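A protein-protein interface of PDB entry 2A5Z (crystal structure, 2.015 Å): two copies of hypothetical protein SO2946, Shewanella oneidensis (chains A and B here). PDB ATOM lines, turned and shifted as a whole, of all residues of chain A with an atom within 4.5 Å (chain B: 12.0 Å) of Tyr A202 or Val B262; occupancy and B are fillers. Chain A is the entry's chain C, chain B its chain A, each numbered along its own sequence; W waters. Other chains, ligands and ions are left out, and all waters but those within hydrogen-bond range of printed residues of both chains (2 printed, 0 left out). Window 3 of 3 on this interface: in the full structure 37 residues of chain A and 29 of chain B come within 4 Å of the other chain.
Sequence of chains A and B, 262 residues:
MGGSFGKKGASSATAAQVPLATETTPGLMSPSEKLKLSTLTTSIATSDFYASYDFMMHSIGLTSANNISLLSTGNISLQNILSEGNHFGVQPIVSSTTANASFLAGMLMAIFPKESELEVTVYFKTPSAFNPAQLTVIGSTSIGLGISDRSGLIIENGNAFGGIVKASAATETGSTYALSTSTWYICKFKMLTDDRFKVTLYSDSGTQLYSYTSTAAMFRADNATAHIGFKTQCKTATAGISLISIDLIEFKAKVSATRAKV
NZ of Lys A188 lies within salt-bridge range of O of Val B262 (2.7 Å).
The backbone NH (N) of Tyr A202 sits at hydrogen-bond distance from the backbone carbonyl oxygen (O) of Ile A186, at 2.7 Å. The backbone carbonyl oxygen (O) of Lys A188 sits at hydrogen-bond distance from the backbone NH (N) of Thr A200 (2.9 Å).
Thr A121 touches Val B262. Ile A186 touches Ala B260. Ile A186 touches Val B262. CG of Tyr A202 touches CG1 of Val B262, at 3.7 Å. Asp A204 touches Ala B260. Gly A206 touches Ala B260 (N to CB, 3.6 Å).
Of chain B, only Val B262 comes within 4 Å of Thr A121. No residue of chain B comes within 4 Å of Tyr A185. Of chain B, only Ala B260 and Val B262 come within 4 Å of Ile A186. Of chain B, only Val B262 comes within 4 Å of Lys A188. No residue of chain B comes within 4 Å of Thr A200. Of chain B, only Val B262 (3.7 Å) comes within 4 Å of Tyr A202. No residue of chain B comes within 4 Å of Ser A203. Printed residues of chain B within 4 Å of Asp A204: Ala B260 (3.6 Å). No residue of chain B comes within 4 Å of Gln A208. No residue of chain B comes within 4 Å of Leu A209. Ala B257 touches none of the printed residues of chain A. Arg B259 touches none of the printed residues of chain A. Printed residues of chain A within 4 Å of Ala B260: Ile A186 (3.9 Å), Asp A204 (3.6 Å) and Gly A206 (3.6 Å). Val B262 touches just these residues of chain A: Thr A121 (3.8 Å), Ile A186 (3.9 Å), Lys A188 (2.7 Å) and Tyr A202 (3.7 Å). The nearest residue of chain B that does not touch Tyr A202 is Lys B261 (6.5 Å). The nearest residue of chain A that does not touch Val B262 is Gly A206 (4.03 Å). The nearest printed residue of chain B that does not touch Asp A204 is Arg B259 (5.3 Å).
Of the 7 printed residues of chain B, 2 touch a printed residue of chain A. Printed residues of chain B that touch a printed residue of chain A: Ala B260 and Val B262. Hydrophobic or aromatic side chains of chain B that line the printed part of chain A: Ala B260 and Val B262. Along chain B the printed residues that touch a printed residue of chain A span positions 260 to 262. Of the 13 printed residues of chain A, 6 touch a printed residue of chain B. Among the printed residues, no Asp or Glu carboxylate lies within 4 Å of a Lys or Arg side-chain nitrogen of the other chain.
No position is printed for both chains.
Water W2 lies within hydrogen-bond range of O of Asp A204 and N of Ala B260. Water W1 bridges the backbone carbonyl oxygen (O) of Gly A206 (2.7 Å) and the backbone carbonyl oxygen (O) of Lys B261 (3.3 Å).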
ATOM      1  N   THR A 121      16.434  -6.768  25.903  1.00  0.00           N
ATOM      2  CA  THR A 121      15.681  -5.757  25.177  1.00  0.00           C
ATOM      3  C   THR A 121      16.358  -4.395  25.320  1.00  0.00           C
ATOM      4  O   THR A 121      16.722  -4.004  26.425  1.00  0.00           O
ATOM      5  CB  THR A 121      14.218  -5.688  25.653  1.00  0.00           C
ATOM      6  OG1 THR A 121      13.654  -7.012  25.653  1.00  0.00           O
ATOM      7  CG2 THR A 121      13.389  -4.798  24.730  1.00  0.00           C
ATOM      8  N   TYR A 185      14.137   3.026  18.116  1.00  0.00           N
ATOM      9  CA  TYR A 185      13.932   1.629  17.722  1.00  0.00           C
ATOM     10  C   TYR A 185      13.962   0.761  18.976  1.00  0.00           C
ATOM     11  O   TYR A 185      14.491   1.177  20.010  1.00  0.00           O
ATOM     12  CB  TYR A 185      15.043   1.159  16.764  1.00  0.00           C
ATOM     13  CG  TYR A 185      15.002   1.768  15.382  1.00  0.00           C
ATOM     14  CD1 TYR A 185      14.084   1.321  14.431  1.00  0.00           C
ATOM     15  CD2 TYR A 185      15.879   2.792  15.022  1.00  0.00           C
ATOM     16  CE1 TYR A 185      14.029   1.887  13.156  1.00  0.00           C
ATOM     17  CE2 TYR A 185      15.842   3.363  13.741  1.00  0.00           C
ATOM     18  CZ  TYR A 185      14.913   2.903  12.818  1.00  0.00           C
ATOM     19  OH  TYR A 185      14.867   3.446  11.558  1.00  0.00           O
ATOM     20  N   ILE A 186      13.397  -0.438  18.884  1.00  0.00           N
ATOM     21  CA  ILE A 186      13.512  -1.432  19.955  1.00  0.00           C
ATOM     22  C   ILE A 186      14.105  -2.703  19.344  1.00  0.00           C
ATOM     23  O   ILE A 186      13.764  -3.071  18.220  1.00  0.00           O
ATOM     24  CB  ILE A 186      12.129  -1.731  20.625  1.00  0.00           C
ATOM     25  CG1 ILE A 186      11.390  -0.429  20.967  1.00  0.00           C
ATOM     26  CG2 ILE A 186      12.289  -2.629  21.881  1.00  0.00           C
ATOM     27  CD1 ILE A 186       9.911  -0.601  21.295  1.00  0.00           C
ATOM     28  N   LYS A 188      14.924  -6.806  20.469  1.00  0.00           N
ATOM     29  CA  LYS A 188      14.967  -7.943  21.369  1.00  0.00           C
ATOM     30  C   LYS A 188      15.913  -9.016  20.823  1.00  0.00           C
ATOM     31  O   LYS A 188      15.824  -9.418  19.659  1.00  0.00           O
ATOM     32  CB  LYS A 188      13.562  -8.499  21.606  1.00  0.00           C
ATOM     33  CG  LYS A 188      13.502  -9.677  22.577  1.00  0.00           C
ATOM     34  CD  LYS A 188      12.129  -9.792  23.229  1.00  0.00           C
ATOM     35  CE  LYS A 188      11.017 -10.002  22.221  1.00  0.00           C
ATOM     36  NZ  LYS A 188       9.813 -10.528  22.908  1.00  0.00           N
ATOM     37  N   THR A 200      15.055  -9.392  16.900  1.00  0.00           N
ATOM     38  CA  THR A 200      13.914  -8.720  16.296  1.00  0.00           C
ATOM     39  C   THR A 200      14.035  -7.229  16.517  1.00  0.00           C
ATOM     40  O   THR A 200      14.242  -6.779  17.650  1.00  0.00           O
ATOM     41  CB  THR A 200      12.583  -9.239  16.868  1.00  0.00           C
ATOM     42  OG1 THR A 200      12.535 -10.659  16.717  1.00  0.00           O
ATOM     43  CG2 THR A 200      11.395  -8.623  16.135  1.00  0.00           C
ATOM     44  N   LEU A 201      13.926  -6.477  15.428  1.00  0.00           N
ATOM     45  CA  LEU A 201      13.893  -5.020  15.473  1.00  0.00           C
ATOM     46  C   LEU A 201      12.452  -4.518  15.322  1.00  0.00           C
ATOM     47  O   LEU A 201      11.700  -4.996  14.467  1.00  0.00           O
ATOM     48  CB  LEU A 201      14.784  -4.444  14.371  1.00  0.00           C
ATOM     49  CG  LEU A 201      14.895  -2.934  14.196  1.00  0.00           C
ATOM     50  CD1 LEU A 201      15.814  -2.303  15.257  1.00  0.00           C
ATOM     51  CD2 LEU A 201      15.384  -2.636  12.781  1.00  0.00           C
ATOM     52  N   TYR A 202      12.071  -3.572  16.177  1.00  0.00           N
ATOM     53  CA  TYR A 202      10.737  -2.994  16.181  1.00  0.00           C
ATOM     54  C   TYR A 202      10.822  -1.480  16.024  1.00  0.00           C
ATOM     55  O   TYR A 202      11.864  -0.860  16.299  1.00  0.00           O
ATOM     56  CB  TYR A 202      10.002  -3.286  17.498  1.00  0.00           C
ATOM     57  CG  TYR A 202      10.007  -4.724  17.971  1.00  0.00           C
ATOM     58  CD1 TYR A 202       8.901  -5.553  17.752  1.00  0.00           C
ATOM     59  CD2 TYR A 202      11.094  -5.244  18.672  1.00  0.00           C
ATOM     60  CE1 TYR A 202       8.881  -6.875  18.210  1.00  0.00           C
ATOM     61  CE2 TYR A 202      11.096  -6.575  19.127  1.00  0.00           C
ATOM     62  CZ  TYR A 202       9.984  -7.380  18.892  1.00  0.00           C
ATOM     63  OH  TYR A 202       9.980  -8.682  19.330  1.00  0.00           O
ATOM     64  N   SER A 203       9.710  -0.885  15.609  1.00  0.00           N
ATOM     65  CA  SER A 203       9.554   0.563  15.665  1.00  0.00           C
ATOM     66  C   SER A 203       9.334   0.971  17.127  1.00  0.00           C
ATOM     67  O   SER A 203       9.159   0.111  18.005  1.00  0.00           O
ATOM     68  CB  SER A 203       8.352   0.984  14.824  1.00  0.00           C
ATOM     69  OG  SER A 203       7.155   0.634  15.493  1.00  0.00           O
ATOM     70  N   ASP A 204       9.316   2.277  17.385  1.00  0.00           N
ATOM     71  CA  ASP A 204       9.107   2.790  18.744  1.00  0.00           C
ATOM     72  C   ASP A 204       7.710   2.479  19.313  1.00  0.00           C
ATOM     73  O   ASP A 204       7.490   2.610  20.517  1.00  0.00           O
ATOM     74  CB  ASP A 204       9.390   4.297  18.805  1.00  0.00           C
ATOM     75  CG  ASP A 204       9.786   4.762  20.200  1.00  0.00           C
ATOM     76  OD1 ASP A 204      10.250   3.923  21.008  1.00  0.00           O
ATOM     77  OD2 ASP A 204       9.661   5.977  20.481  1.00  0.00           O
ATOM     78  N   GLY A 206       6.438  -0.622  18.857  1.00  0.00           N
ATOM     79  CA  GLY A 206       6.470  -2.079  19.005  1.00  0.00           C
ATOM     80  C   GLY A 206       6.040  -2.874  17.782  1.00  0.00           C
ATOM     81  O   GLY A 206       5.781  -4.070  17.877  1.00  0.00           O
ATOM     82  N   THR A 207       5.969  -2.213  16.630  1.00  0.00           N
ATOM     83  CA  THR A 207       5.632  -2.879  15.373  1.00  0.00           C
ATOM     84  C   THR A 207       6.866  -3.590  14.822  1.00  0.00           C
ATOM     85  O   THR A 207       7.921  -2.980  14.703  1.00  0.00           O
ATOM     86  CB  THR A 207       5.084  -1.856  14.350  1.00  0.00           C
ATOM     87  OG1 THR A 207       3.921  -1.236  14.900  1.00  0.00           O
ATOM     88  CG2 THR A 207       4.704  -2.530  13.032  1.00  0.00           C
ATOM     89  N   GLN A 208       6.746  -4.877  14.500  1.00  0.00           N
ATOM     90  CA  GLN A 208       7.909  -5.618  14.014  1.00  0.00           C
ATOM     91  C   GLN A 208       8.347  -5.118  12.638  1.00  0.00           C
ATOM     92  O   GLN A 208       7.542  -5.015  11.719  1.00  0.00           O
ATOM     93  CB  GLN A 208       7.683  -7.133  14.000  1.00  0.00           C
ATOM     94  CG  GLN A 208       8.920  -7.911  13.538  1.00  0.00           C
ATOM     95  CD  GLN A 208       8.815  -9.399  13.764  1.00  0.00           C
ATOM     96  OE1 GLN A 208       8.493  -9.858  14.863  1.00  0.00           O
ATOM     97  NE2 GLN A 208       9.094 -10.167  12.722  1.00  0.00           N
ATOM     98  N   LEU A 209       9.638  -4.813  12.530  1.00  0.00           N
ATOM     99  CA  LEU A 209      10.235  -4.266  11.312  1.00  0.00           C
ATOM    100  C   LEU A 209      11.153  -5.276  10.632  1.00  0.00           C
ATOM    101  O   LEU A 209      11.261  -5.305   9.404  1.00  0.00           O
ATOM    102  CB  LEU A 209      11.037  -2.996  11.643  1.00  0.00           C
ATOM    103  CG  LEU A 209      10.282  -1.735  12.083  1.00  0.00           C
ATOM    104  CD1 LEU A 209      11.277  -0.596  12.381  1.00  0.00           C
ATOM    105  CD2 LEU A 209       9.259  -1.312  11.034  1.00  0.00           C
ATOM    106  N   ILE B  44      12.967   0.809  35.848  1.00  0.00           N
ATOM    107  CA  ILE B  44      12.319   1.302  34.627  1.00  0.00           C
ATOM    108  C   ILE B  44      11.181   2.221  35.038  1.00  0.00           C
ATOM    109  O   ILE B  44      10.273   1.799  35.756  1.00  0.00           O
ATOM    110  CB  ILE B  44      11.736   0.165  33.744  1.00  0.00           C
ATOM    111  CG1 ILE B  44      12.791  -0.893  33.452  1.00  0.00           C
ATOM    112  CG2 ILE B  44      11.184   0.738  32.420  1.00  0.00           C
ATOM    113  CD1 ILE B  44      12.357  -1.945  32.464  1.00  0.00           C
ATOM    114  N   ALA B 257       6.668   8.208  31.076  1.00  0.00           N
ATOM    115  CA  ALA B 257       7.647   7.282  30.502  1.00  0.00           C
ATOM    116  C   ALA B 257       7.028   5.974  30.004  1.00  0.00           C
ATOM    117  O   ALA B 257       7.440   4.881  30.407  1.00  0.00           O
ATOM    118  CB  ALA B 257       8.761   7.003  31.497  1.00  0.00           C
ATOM    119  N   THR B 258       6.058   6.097  29.105  1.00  0.00           N
ATOM    120  CA  THR B 258       5.403   4.942  28.504  1.00  0.00           C
ATOM    121  C   THR B 258       6.109   4.489  27.225  1.00  0.00           C
ATOM    122  O   THR B 258       6.006   5.151  26.184  1.00  0.00           O
ATOM    123  CB  THR B 258       3.936   5.269  28.158  1.00  0.00           C
ATOM    124  OG1 THR B 258       3.381   6.116  29.171  1.00  0.00           O
ATOM    125  CG2 THR B 258       3.113   3.999  28.041  1.00  0.00           C
ATOM    126  N   ARG B 259       6.830   3.369  27.288  1.00  0.00           N
ATOM    127  CA  ARG B 259       7.328   2.765  26.047  1.00  0.00           C
ATOM    128  C   ARG B 259       6.686   1.433  25.706  1.00  0.00           C
ATOM    129  O   ARG B 259       6.250   0.698  26.589  1.00  0.00           O
ATOM    130  CB  ARG B 259       8.864   2.682  25.940  1.00  0.00           C
ATOM    131  CG  ARG B 259       9.660   2.676  27.204  1.00  0.00           C
ATOM    132  CD  ARG B 259      10.091   4.085  27.567  1.00  0.00           C
ATOM    133  NE  ARG B 259      10.159   4.161  29.017  1.00  0.00           N
ATOM    134  CZ  ARG B 259      11.258   4.381  29.724  1.00  0.00           C
ATOM    135  NH1 ARG B 259      11.171   4.394  31.048  1.00  0.00           N
ATOM    136  NH2 ARG B 259      12.422   4.616  29.119  1.00  0.00           N
ATOM    137  N   ALA B 260       6.631   1.149  24.408  1.00  0.00           N
ATOM    138  CA  ALA B 260       6.058  -0.081  23.891  1.00  0.00           C
ATOM    139  C   ALA B 260       6.702  -1.296  24.541  1.00  0.00           C
ATOM    140  O   ALA B 260       7.917  -1.346  24.733  1.00  0.00           O
ATOM    141  CB  ALA B 260       6.219  -0.141  22.387  1.00  0.00           C
ATOM    142  N   LYS B 261       5.858  -2.257  24.902  1.00  0.00           N
ATOM    143  CA  LYS B 261       6.306  -3.540  25.407  1.00  0.00           C
ATOM    144  C   LYS B 261       6.466  -4.434  24.191  1.00  0.00           C
ATOM    145  O   LYS B 261       5.701  -4.319  23.227  1.00  0.00           O
ATOM    146  CB  LYS B 261       5.263  -4.133  26.358  1.00  0.00           C
ATOM    147  CG  LYS B 261       4.945  -3.288  27.594  1.00  0.00           C
ATOM    148  CD  LYS B 261       5.911  -3.572  28.750  1.00  0.00           C
ATOM    149  CE  LYS B 261       5.406  -2.982  30.073  1.00  0.00           C
ATOM    150  NZ  LYS B 261       5.387  -1.478  30.085  1.00  0.00           N
ATOM    151  N   VAL B 262       7.482  -5.290  24.211  1.00  0.00           N
ATOM    152  CA  VAL B 262       7.702  -6.255  23.129  1.00  0.00           C
ATOM    153  C   VAL B 262       7.928  -7.657  23.704  1.00  0.00           C
ATOM    154  O   VAL B 262       7.910  -8.654  22.989  1.00  0.00           O
ATOM    155  CB  VAL B 262       8.884  -5.855  22.186  1.00  0.00           C
ATOM    156  CG1 VAL B 262       8.545  -4.605  21.363  1.00  0.00           C
ATOM    157  CG2 VAL B 262      10.194  -5.675  22.964  1.00  0.00           C
ATOM    158  OXT VAL B 262       8.134  -7.827  24.906  1.00  0.00           O
HETATM  159  O   HOH W   1       5.297  -5.487  20.129  1.00  0.00           O
HETATM  160  O   HOH W   2       8.371   2.904  22.884  1.00  0.00           O
